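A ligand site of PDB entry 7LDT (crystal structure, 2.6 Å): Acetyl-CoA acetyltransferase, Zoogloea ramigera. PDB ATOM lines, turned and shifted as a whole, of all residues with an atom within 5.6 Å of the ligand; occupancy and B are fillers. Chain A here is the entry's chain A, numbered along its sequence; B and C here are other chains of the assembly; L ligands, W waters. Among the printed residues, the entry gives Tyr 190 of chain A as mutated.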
ATOM      1  N   SCY A  96      -6.501  20.697  34.074  1.00  0.00           N
ATOM      2  CA  SCY A  96      -5.057  20.844  34.194  1.00  0.00           C
ATOM      3  CB  SCY A  96      -4.565  22.008  33.365  1.00  0.00           C
ATOM      4  SG  SCY A  96      -4.930  21.771  31.624  1.00  0.00           S
ATOM      5  CD  SCY A  96      -6.529  22.291  31.371  1.00  0.00           C
ATOM      6  OCD SCY A  96      -7.220  23.003  32.115  1.00  0.00           O
ATOM      7  CE  SCY A  96      -7.057  21.797  30.059  1.00  0.00           C
ATOM      8  C   SCY A  96      -4.505  21.046  35.654  1.00  0.00           C
ATOM      9  O   SCY A  96      -3.295  20.778  35.885  1.00  0.00           O
ATOM     10  N   LEU A 155      -9.659  19.385  25.899  1.00  0.00           N
ATOM     11  CA  LEU A 155      -9.090  20.577  25.274  1.00  0.00           C
ATOM     12  C   LEU A 155     -10.111  21.506  24.644  1.00  0.00           C
ATOM     13  O   LEU A 155      -9.717  22.470  23.978  1.00  0.00           O
ATOM     14  CB  LEU A 155      -8.051  20.167  24.227  1.00  0.00           C
ATOM     15  CG  LEU A 155      -6.968  19.202  24.696  1.00  0.00           C
ATOM     16  CD1 LEU A 155      -6.061  18.861  23.535  1.00  0.00           C
ATOM     17  CD2 LEU A 155      -6.176  19.803  25.842  1.00  0.00           C
ATOM     18  N   HIS A 163     -11.179  25.533  21.038  1.00  0.00           N
ATOM     19  CA  HIS A 163     -10.037  24.926  21.702  1.00  0.00           C
ATOM     20  C   HIS A 163      -9.449  25.885  22.730  1.00  0.00           C
ATOM     21  O   HIS A 163      -9.713  27.093  22.728  1.00  0.00           O
ATOM     22  CB  HIS A 163      -8.987  24.540  20.665  1.00  0.00           C
ATOM     23  CG  HIS A 163      -7.973  23.547  21.158  1.00  0.00           C
ATOM     24  ND1 HIS A 163      -6.847  23.928  21.864  1.00  0.00           N
ATOM     25  CD2 HIS A 163      -7.902  22.210  21.028  1.00  0.00           C
ATOM     26  CE1 HIS A 163      -6.132  22.861  22.155  1.00  0.00           C
ATOM     27  NE2 HIS A 163      -6.745  21.797  21.655  1.00  0.00           N
ATOM     28  N   MET A 164      -8.617  25.334  23.623  1.00  0.00           N
ATOM     29  CA  MET A 164      -7.930  26.152  24.613  1.00  0.00           C
ATOM     30  C   MET A 164      -6.946  27.122  23.971  1.00  0.00           C
ATOM     31  O   MET A 164      -6.619  28.148  24.582  1.00  0.00           O
ATOM     32  CB  MET A 164      -7.214  25.269  25.629  1.00  0.00           C
ATOM     33  CG  MET A 164      -8.125  24.364  26.450  1.00  0.00           C
ATOM     34  SD  MET A 164      -9.117  25.249  27.669  1.00  0.00           S
ATOM     35  CE  MET A 164     -10.649  25.518  26.774  1.00  0.00           C
ATOM     36  N   GLY A 165      -6.453  26.817  22.772  1.00  0.00           N
ATOM     37  CA  GLY A 165      -5.593  27.759  22.075  1.00  0.00           C
ATOM     38  C   GLY A 165      -6.292  29.042  21.694  1.00  0.00           C
ATOM     39  O   GLY A 165      -5.664  30.094  21.563  1.00  0.00           O
ATOM     40  N   TYR A 190      12.511  26.522  25.762  1.00  0.00           N
ATOM     41  CA  TYR A 190      13.290  25.399  25.235  1.00  0.00           C
ATOM     42  C   TYR A 190      14.749  25.472  25.666  1.00  0.00           C
ATOM     43  O   TYR A 190      15.348  24.442  26.018  1.00  0.00           O
ATOM     44  CB  TYR A 190      13.184  25.363  23.716  1.00  0.00           C
ATOM     45  CG  TYR A 190      11.926  24.688  23.196  1.00  0.00           C
ATOM     46  CD1 TYR A 190      11.821  23.311  23.158  1.00  0.00           C
ATOM     47  CD2 TYR A 190      10.855  25.448  22.742  1.00  0.00           C
ATOM     48  CE1 TYR A 190      10.685  22.683  22.684  1.00  0.00           C
ATOM     49  CE2 TYR A 190       9.705  24.838  22.264  1.00  0.00           C
ATOM     50  CZ  TYR A 190       9.629  23.451  22.235  1.00  0.00           C
ATOM     51  OH  TYR A 190       8.497  22.832  21.757  1.00  0.00           O
ATOM     52  N   ARG A 227      13.545  19.816  22.892  1.00  0.00           N
ATOM     53  CA  ARG A 227      14.248  19.971  21.623  1.00  0.00           C
ATOM     54  C   ARG A 227      15.637  20.540  21.856  1.00  0.00           C
ATOM     55  O   ARG A 227      15.819  21.456  22.668  1.00  0.00           O
ATOM     56  CB  ARG A 227      13.482  20.890  20.679  1.00  0.00           C
ATOM     57  CG  ARG A 227      12.231  20.297  20.037  1.00  0.00           C
ATOM     58  CD  ARG A 227      11.672  21.251  18.998  1.00  0.00           C
ATOM     59  NE  ARG A 227      10.515  20.711  18.285  1.00  0.00           N
ATOM     60  CZ  ARG A 227      10.584  20.102  17.109  1.00  0.00           C
ATOM     61  NH1 ARG A 227      11.760  19.944  16.515  1.00  0.00           N
ATOM     62  NH2 ARG A 227       9.485  19.641  16.540  1.00  0.00           N
ATOM     63  N   ALA A 230      16.646  24.659  19.460  1.00  0.00           N
ATOM     64  CA  ALA A 230      15.404  25.246  18.954  1.00  0.00           C
ATOM     65  C   ALA A 230      15.682  26.667  18.485  1.00  0.00           C
ATOM     66  O   ALA A 230      16.021  27.539  19.286  1.00  0.00           O
ATOM     67  CB  ALA A 230      14.322  25.218  20.032  1.00  0.00           C
ATOM     68  N   THR A 231      15.549  26.906  17.177  1.00  0.00           N
ATOM     69  CA  THR A 231      15.896  28.191  16.598  1.00  0.00           C
ATOM     70  C   THR A 231      14.671  29.103  16.525  1.00  0.00           C
ATOM     71  O   THR A 231      13.531  28.644  16.465  1.00  0.00           O
ATOM     72  CB  THR A 231      16.484  28.011  15.200  1.00  0.00           C
ATOM     73  OG1 THR A 231      15.426  27.718  14.272  1.00  0.00           O
ATOM     74  CG2 THR A 231      17.479  26.870  15.198  1.00  0.00           C
ATOM     75  N   SER A 234      12.897  28.873  12.804  1.00  0.00           N
ATOM     76  CA  SER A 234      11.915  27.814  12.618  1.00  0.00           C
ATOM     77  C   SER A 234      10.668  28.037  13.472  1.00  0.00           C
ATOM     78  O   SER A 234       9.606  27.500  13.134  1.00  0.00           O
ATOM     79  CB  SER A 234      12.538  26.461  12.954  1.00  0.00           C
ATOM     80  OG  SER A 234      12.884  26.370  14.328  1.00  0.00           O
ATOM     81  N   MET A 235      10.783  28.821  14.545  1.00  0.00           N
ATOM     82  CA  MET A 235       9.622  29.153  15.361  1.00  0.00           C
ATOM     83  C   MET A 235       8.752  30.211  14.697  1.00  0.00           C
ATOM     84  O   MET A 235       7.526  30.178  14.852  1.00  0.00           O
ATOM     85  CB  MET A 235      10.080  29.643  16.743  1.00  0.00           C
ATOM     86  CG  MET A 235       8.970  29.765  17.777  1.00  0.00           C
ATOM     87  SD  MET A 235       8.486  28.173  18.461  1.00  0.00           S
ATOM     88  CE  MET A 235      10.064  27.574  19.077  1.00  0.00           C
ATOM     89  N   LEU A 238       6.346  28.886  11.562  1.00  0.00           N
ATOM     90  CA  LEU A 238       5.190  28.032  11.795  1.00  0.00           C
ATOM     91  C   LEU A 238       3.895  28.819  11.621  1.00  0.00           C
ATOM     92  O   LEU A 238       3.811  29.996  11.981  1.00  0.00           O
ATOM     93  CB  LEU A 238       5.233  27.424  13.201  1.00  0.00           C
ATOM     94  CG  LEU A 238       6.472  26.595  13.533  1.00  0.00           C
ATOM     95  CD1 LEU A 238       6.433  26.118  14.977  1.00  0.00           C
ATOM     96  CD2 LEU A 238       6.589  25.419  12.587  1.00  0.00           C
ATOM     97  N   ALA A 241      -2.005  27.685  14.713  1.00  0.00           N
ATOM     98  CA  ALA A 241      -2.634  26.375  14.839  1.00  0.00           C
ATOM     99  C   ALA A 241      -4.132  26.427  15.118  1.00  0.00           C
ATOM    100  O   ALA A 241      -4.793  25.392  15.029  1.00  0.00           O
ATOM    101  CB  ALA A 241      -1.938  25.571  15.946  1.00  0.00           C
ATOM    102  N   PHE A 242      -4.675  27.596  15.454  1.00  0.00           N
ATOM    103  CA  PHE A 242      -6.097  27.671  15.808  1.00  0.00           C
ATOM    104  C   PHE A 242      -6.808  28.731  14.984  1.00  0.00           C
ATOM    105  O   PHE A 242      -7.724  28.416  14.225  1.00  0.00           O
ATOM    106  CB  PHE A 242      -6.253  27.947  17.309  1.00  0.00           C
ATOM    107  CG  PHE A 242      -5.491  26.994  18.180  1.00  0.00           C
ATOM    108  CD1 PHE A 242      -5.988  25.734  18.437  1.00  0.00           C
ATOM    109  CD2 PHE A 242      -4.271  27.359  18.723  1.00  0.00           C
ATOM    110  CE1 PHE A 242      -5.282  24.847  19.237  1.00  0.00           C
ATOM    111  CE2 PHE A 242      -3.562  26.480  19.518  1.00  0.00           C
ATOM    112  CZ  PHE A 242      -4.067  25.224  19.776  1.00  0.00           C
ATOM    113  N   THR A 249       0.741  29.186  17.903  1.00  0.00           N
ATOM    114  CA  THR A 249       1.161  28.137  16.994  1.00  0.00           C
ATOM    115  C   THR A 249       1.487  26.875  17.793  1.00  0.00           C
ATOM    116  O   THR A 249       1.466  26.868  19.024  1.00  0.00           O
ATOM    117  CB  THR A 249       2.374  28.560  16.159  1.00  0.00           C
ATOM    118  OG1 THR A 249       3.511  28.669  17.016  1.00  0.00           O
ATOM    119  CG2 THR A 249       2.116  29.901  15.490  1.00  0.00           C
ATOM    120  N   ALA A 250       1.821  25.812  17.070  1.00  0.00           N
ATOM    121  CA  ALA A 250       2.250  24.574  17.721  1.00  0.00           C
ATOM    122  C   ALA A 250       3.578  24.754  18.439  1.00  0.00           C
ATOM    123  O   ALA A 250       3.871  23.982  19.364  1.00  0.00           O
ATOM    124  CB  ALA A 250       2.359  23.451  16.701  1.00  0.00           C
ATOM    125  N   GLY A 251       4.378  25.742  18.052  1.00  0.00           N
ATOM    126  CA  GLY A 251       5.670  25.980  18.655  1.00  0.00           C
ATOM    127  C   GLY A 251       5.604  26.739  19.967  1.00  0.00           C
ATOM    128  O   GLY A 251       6.292  26.398  20.921  1.00  0.00           O
ATOM    129  N   ALA A 253       3.092  26.858  21.984  1.00  0.00           N
ATOM    130  CA  ALA A 253       2.056  26.271  22.809  1.00  0.00           C
ATOM    131  C   ALA A 253       2.515  24.907  23.309  1.00  0.00           C
ATOM    132  O   ALA A 253       3.296  24.224  22.637  1.00  0.00           O
ATOM    133  CB  ALA A 253       0.728  26.114  22.038  1.00  0.00           C
ATOM    134  N   SER A 254       2.042  24.534  24.483  1.00  0.00           N
ATOM    135  CA  SER A 254       2.339  23.202  25.011  1.00  0.00           C
ATOM    136  C   SER A 254       1.666  22.141  24.159  1.00  0.00           C
ATOM    137  O   SER A 254       0.625  22.379  23.538  1.00  0.00           O
ATOM    138  CB  SER A 254       1.872  23.083  26.464  1.00  0.00           C
ATOM    139  OG  SER A 254       0.467  23.208  26.565  1.00  0.00           O
ATOM    140  N   GLY A 255       2.277  20.962  24.121  1.00  0.00           N
ATOM    141  CA  GLY A 255       1.804  19.878  23.298  1.00  0.00           C
ATOM    142  C   GLY A 255       0.942  18.889  24.068  1.00  0.00           C
ATOM    143  O   GLY A 255       0.464  19.152  25.173  1.00  0.00           O
ATOM    144  N   LEU A 256       0.732  17.738  23.444  1.00  0.00           N
ATOM    145  CA  LEU A 256       0.002  16.625  24.044  1.00  0.00           C
ATOM    146  C   LEU A 256       0.997  15.591  24.534  1.00  0.00           C
ATOM    147  O   LEU A 256       1.913  15.213  23.802  1.00  0.00           O
ATOM    148  CB  LEU A 256      -0.963  16.015  23.030  1.00  0.00           C
ATOM    149  CG  LEU A 256      -1.673  17.028  22.137  1.00  0.00           C
ATOM    150  CD1 LEU A 256      -2.471  16.323  21.044  1.00  0.00           C
ATOM    151  CD2 LEU A 256      -2.586  17.926  22.965  1.00  0.00           C
ATOM    152  N   MET A 295      -9.285  31.880  30.306  1.00  0.00           N
ATOM    153  CA  MET A 295      -8.949  30.899  31.341  1.00  0.00           C
ATOM    154  C   MET A 295      -7.462  30.913  31.704  1.00  0.00           C
ATOM    155  O   MET A 295      -7.109  30.432  32.785  1.00  0.00           O
ATOM    156  CB  MET A 295      -9.367  29.502  30.874  1.00  0.00           C
ATOM    157  CG  MET A 295      -8.556  28.938  29.733  1.00  0.00           C
ATOM    158  SD  MET A 295      -7.147  27.960  30.302  1.00  0.00           S
ATOM    159  CE  MET A 295      -6.202  27.850  28.780  1.00  0.00           C
ATOM    160  N   ALA A 325       0.988  26.710  29.771  1.00  0.00           N
ATOM    161  CA  ALA A 325       0.027  26.155  28.823  1.00  0.00           C
ATOM    162  C   ALA A 325       0.202  26.781  27.446  1.00  0.00           C
ATOM    163  O   ALA A 325       0.271  26.083  26.437  1.00  0.00           O
ATOM    164  CB  ALA A 325      -1.403  26.359  29.334  1.00  0.00           C
ATOM    165  N   PHE A 326       0.287  28.113  27.398  1.00  0.00           N
ATOM    166  CA  PHE A 326       0.539  28.833  26.166  1.00  0.00           C
ATOM    167  C   PHE A 326       1.454  30.013  26.457  1.00  0.00           C
ATOM    168  O   PHE A 326       1.469  30.541  27.575  1.00  0.00           O
ATOM    169  CB  PHE A 326      -0.761  29.341  25.516  1.00  0.00           C
ATOM    170  CG  PHE A 326      -1.732  28.251  25.178  1.00  0.00           C
ATOM    171  CD1 PHE A 326      -2.686  27.838  26.093  1.00  0.00           C
ATOM    172  CD2 PHE A 326      -1.703  27.650  23.928  1.00  0.00           C
ATOM    173  CE1 PHE A 326      -3.575  26.831  25.783  1.00  0.00           C
ATOM    174  CE2 PHE A 326      -2.602  26.643  23.609  1.00  0.00           C
ATOM    175  CZ  PHE A 326      -3.532  26.233  24.530  1.00  0.00           C
ATOM    176  N   HIS A 355       2.936  18.812  28.475  1.00  0.00           N
ATOM    177  CA  HIS A 355       1.753  19.146  29.273  1.00  0.00           C
ATOM    178  C   HIS A 355       0.811  17.944  29.356  1.00  0.00           C
ATOM    179  O   HIS A 355      -0.197  17.879  28.644  1.00  0.00           O
ATOM    180  CB  HIS A 355       1.026  20.364  28.682  1.00  0.00           C
ATOM    181  CG  HIS A 355       0.040  20.998  29.618  1.00  0.00           C
ATOM    182  ND1 HIS A 355      -0.232  20.490  30.866  1.00  0.00           N
ATOM    183  CD2 HIS A 355      -0.725  22.106  29.483  1.00  0.00           C
ATOM    184  CE1 HIS A 355      -1.138  21.258  31.461  1.00  0.00           C
ATOM    185  NE2 HIS A 355      -1.442  22.242  30.638  1.00  0.00           N
ATOM    186  N   ILE A 357      -2.075  16.853  30.987  1.00  0.00           N
ATOM    187  CA  ILE A 357      -3.052  17.684  31.690  1.00  0.00           C
ATOM    188  C   ILE A 357      -3.252  17.264  33.140  1.00  0.00           C
ATOM    189  O   ILE A 357      -2.958  18.021  34.061  1.00  0.00           O
ATOM    190  CB  ILE A 357      -4.384  17.727  30.926  1.00  0.00           C
ATOM    191  CG1 ILE A 357      -4.753  16.360  30.373  1.00  0.00           C
ATOM    192  CG2 ILE A 357      -4.297  18.730  29.786  1.00  0.00           C
ATOM    193  CD1 ILE A 357      -6.021  16.372  29.535  1.00  0.00           C
ATOM    194  N   CYS A 385      -3.063  27.216  35.196  1.00  0.00           N
ATOM    195  CA  CYS A 385      -4.364  27.656  34.704  1.00  0.00           C
ATOM    196  C   CYS A 385      -5.202  26.428  34.364  1.00  0.00           C
ATOM    197  O   CYS A 385      -4.679  25.357  34.036  1.00  0.00           O
ATOM    198  CB  CYS A 385      -4.224  28.559  33.485  1.00  0.00           C
ATOM    199  SG  CYS A 385      -3.565  27.783  32.008  1.00  0.00           S
ATOM    200  N   ILE A 386      -6.528  26.580  34.452  1.00  0.00           N
ATOM    201  CA  ILE A 386      -7.456  25.472  34.320  1.00  0.00           C
ATOM    202  C   ILE A 386      -8.526  25.846  33.300  1.00  0.00           C
ATOM    203  O   ILE A 386      -9.062  26.949  33.334  1.00  0.00           O
ATOM    204  CB  ILE A 386      -8.093  25.108  35.673  1.00  0.00           C
ATOM    205  CG1 ILE A 386      -7.001  24.759  36.690  1.00  0.00           C
ATOM    206  CG2 ILE A 386      -9.072  23.962  35.511  1.00  0.00           C
ATOM    207  CD1 ILE A 386      -7.476  24.829  38.123  1.00  0.00           C
ATOM    208  N   GLY A 387      -8.832  24.900  32.403  1.00  0.00           N
ATOM    209  CA  GLY A 387      -9.903  25.136  31.450  1.00  0.00           C
ATOM    210  C   GLY A 387     -11.226  25.382  32.154  1.00  0.00           C
ATOM    211  O   GLY A 387     -11.463  24.944  33.280  1.00  0.00           O
ATOM    212  N   MET B 141      -5.634  12.357  15.731  1.00  0.00           N
ATOM    213  CA  MET B 141      -6.252  13.429  16.513  1.00  0.00           C
ATOM    214  C   MET B 141      -7.485  13.934  15.775  1.00  0.00           C
ATOM    215  O   MET B 141      -7.500  14.004  14.537  1.00  0.00           O
ATOM    216  CB  MET B 141      -5.254  14.572  16.738  1.00  0.00           C
ATOM    217  CG  MET B 141      -5.755  15.682  17.615  1.00  0.00           C
ATOM    218  SD  MET B 141      -4.453  16.882  17.959  1.00  0.00           S
ATOM    219  CE  MET B 141      -3.872  17.235  16.304  1.00  0.00           C
ATOM    220  N   LYS C 215       3.007  16.906   0.023  1.00  0.00           N
ATOM    221  CA  LYS C 215       4.407  17.306   0.071  1.00  0.00           C
ATOM    222  C   LYS C 215       5.185  16.878  -1.173  1.00  0.00           C
ATOM    223  O   LYS C 215       6.413  16.804  -1.122  1.00  0.00           O
ATOM    224  CB  LYS C 215       5.115  16.786   1.324  1.00  0.00           C
ATOM    225  CG  LYS C 215       4.405  16.988   2.647  1.00  0.00           C
ATOM    226  CD  LYS C 215       5.312  16.508   3.783  1.00  0.00           C
ATOM    227  CE  LYS C 215       4.678  16.662   5.156  1.00  0.00           C
ATOM    228  NZ  LYS C 215       5.592  16.172   6.228  1.00  0.00           N
HETATM  229  N1  LIG L   1      10.090  24.460  16.960  1.00  0.00           N
HETATM  230  C1  LIG L   1      10.121  24.323  15.644  1.00  0.00           C
HETATM  231  N2  LIG L   1       9.173  23.687  14.966  1.00  0.00           N
HETATM  232  C2  LIG L   1       8.147  23.140  15.609  1.00  0.00           C
HETATM  233  C3  LIG L   1       8.098  23.266  17.010  1.00  0.00           C
HETATM  234  C4  LIG L   1       9.100  23.942  17.673  1.00  0.00           C
HETATM  235  N3  LIG L   1       9.009  24.050  19.045  1.00  0.00           N
HETATM  236  N4  LIG L   1       6.989  22.655  17.464  1.00  0.00           N
HETATM  237  C5  LIG L   1       6.356  22.158  16.466  1.00  0.00           C
HETATM  238  N5  LIG L   1       7.009  22.421  15.293  1.00  0.00           N
HETATM  239  C6  LIG L   1       6.532  21.986  13.980  1.00  0.00           C
HETATM  240  C7  LIG L   1       6.372  20.425  13.981  1.00  0.00           C
HETATM  241  O1  LIG L   1       7.567  19.693  13.648  1.00  0.00           O
HETATM  242  C8  LIG L   1       5.290  20.262  12.874  1.00  0.00           C
HETATM  243  O2  LIG L   1       5.838  20.463  11.570  1.00  0.00           O
HETATM  244  P1  LIG L   1       5.931  19.058  10.775  1.00  0.00           P
HETATM  245  O3  LIG L   1       4.662  18.841  10.040  1.00  0.00           O
HETATM  246  O4  LIG L   1       7.166  19.150   9.731  1.00  0.00           O
HETATM  247  O5  LIG L   1       6.171  17.830  11.806  1.00  0.00           O
HETATM  248  C9  LIG L   1       4.343  21.421  13.232  1.00  0.00           C
HETATM  249  O6  LIG L   1       5.178  22.463  13.734  1.00  0.00           O
HETATM  250  C10 LIG L   1       3.339  21.003  14.311  1.00  0.00           C
HETATM  251  O7  LIG L   1       2.980  19.625  14.241  1.00  0.00           O
HETATM  252  P2  LIG L   1       2.786  19.104  15.764  1.00  0.00           P
HETATM  253  O8  LIG L   1       4.051  19.337  16.504  1.00  0.00           O
HETATM  254  O9  LIG L   1       2.507  17.502  15.738  1.00  0.00           O
HETATM  255  O10 LIG L   1       1.620  19.911  16.553  1.00  0.00           O
HETATM  256  P3  LIG L   1       0.121  19.501  16.112  1.00  0.00           P
HETATM  257  O11 LIG L   1      -0.074  19.884  14.692  1.00  0.00           O
HETATM  258  O12 LIG L   1      -0.104  17.902  16.271  1.00  0.00           O
HETATM  259  O13 LIG L   1      -0.990  20.265  17.018  1.00  0.00           O
HETATM  260  C11 LIG L   1      -1.337  21.774  18.887  1.00  0.00           C
HETATM  261  C12 LIG L   1      -0.340  21.208  17.877  1.00  0.00           C
HETATM  262  C13 LIG L   1      -0.828  23.109  19.417  1.00  0.00           C
HETATM  263  C14 LIG L   1      -2.681  22.002  18.193  1.00  0.00           C
HETATM  264  C15 LIG L   1      -1.509  20.780  20.061  1.00  0.00           C
HETATM  265  O14 LIG L   1      -0.213  20.493  20.590  1.00  0.00           O
HETATM  266  C16 LIG L   1      -2.410  21.294  21.161  1.00  0.00           C
HETATM  267  O15 LIG L   1      -3.605  21.181  21.059  1.00  0.00           O
HETATM  268  N6  LIG L   1      -1.903  21.854  22.288  1.00  0.00           N
HETATM  269  C17 LIG L   1      -2.834  22.327  23.323  1.00  0.00           C
HETATM  270  C18 LIG L   1      -2.337  21.973  24.732  1.00  0.00           C
HETATM  271  C19 LIG L   1      -3.360  22.392  25.762  1.00  0.00           C
HETATM  272  O16 LIG L   1      -4.443  22.805  25.406  1.00  0.00           O
HETATM  273  N7  LIG L   1      -3.069  22.300  27.080  1.00  0.00           N
HETATM  274  C20 LIG L   1      -4.036  22.697  28.098  1.00  0.00           C
HETATM  275  C21 LIG L   1      -4.105  24.223  28.195  1.00  0.00           C
HETATM  276  S1  LIG L   1      -4.787  24.725  29.808  1.00  0.00           S
HETATM  277  O   HOH W   1      -5.263  19.903  19.083  1.00  0.00           O
HETATM  278  O   HOH W   2       2.321  22.237  20.464  1.00  0.00           O
HETATM  279  O   HOH W   3       0.977  18.862  12.479  1.00  0.00           O
HETATM  280  O   HOH W   4      -2.095  19.080  26.433  1.00  0.00           O
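The backbone NH of Gly 251 lies close to the side-chain hydroxyl of Thr 249 (3.2 Å).
The side-chain hydroxyl (OG) of Ser 254 lies within hydrogen-bond range of the backbone carbonyl oxygen (O) of Ala 325 (2.9 Å).
A ring nitrogen (ND1) of His 163 is in hydrogen-bond range of the backbone NH of Gly 165.
A ring nitrogen (NE2) of His 355 sits at hydrogen-bond distance from SG of SCY 96, at 3.7 Å.
O of Leu 155 is in hydrogen-bond range of N of Met 164.
OCD of SCY 96 is in hydrogen-bond range of N of Gly 387.
OG of Ser 234 is in hydrogen-bond range of OG1 of Thr 231 (2.9 Å).
Water W1 bridges an oxygen (O15) of the ligand (2.9 Å) and the side-chain sulfur (SD) of Met 141 of chain B (3.3 Å).
Water W2 lies within hydrogen-bond range of the backbone carbonyl oxygen of Ala 250 (2.6 Å), an oxygen (O14) of the ligand (3.1 Å) and the backbone carbonyl oxygen of Ala 253 (3.1 Å).
Water W4 lies within hydrogen-bond range of the backbone carbonyl oxygen of Gly 255 (2.9 Å), the backbone carbonyl oxygen of His 355 (3.2 Å) and a nitrogen (N7) of the ligand (3.4 Å).
Residues that only touch the ligand: Leu 155, Met 164, Ser 234, Met 235, Leu 238, Phe 242, Ala 250, Gly 251, Gly 255, Leu 256, Met 295, Ala 325, Phe 326, His 355, Cys 385 and Met 141 of chain B.
Hydrophobic or aromatic side chains within 4 Å of the ligand: Leu 155, His 163, Met 164, Tyr 190, Met 235, Leu 238, Phe 242, Ala 250, Leu 256, Met 295, Ala 325, Phe 326, His 355 and Met 141 of chain B.
21 residues have an atom within 4 Å of the ligand: SCY 96, Leu 155, His 163, Met 164, Tyr 190, Arg 227, Ser 234, Met 235, Leu 238, Phe 242, Ala 250, Gly 251, Ser 254, Gly 255, Leu 256, Met 295, Ala 325, Phe 326, His 355, Cys 385 and Met 141 of chain B.
N6 of the ligand lies within hydrogen-bond range of O of Ser 254, at 2.9 Å.
NH2 of Arg 227 lies within hydrogen-bond range of O1 of the ligand (3.5 Å).
A nitrogen (N3) of the ligand is in hydrogen-bond range of the side-chain hydroxyl of Tyr 190, 3.0 Å away.
SG of SCY 96 lies close to a sulfur (S1) of the ligand, at 3.5 Å.
NE2 of His 163 lies close to O15 of the ligand.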
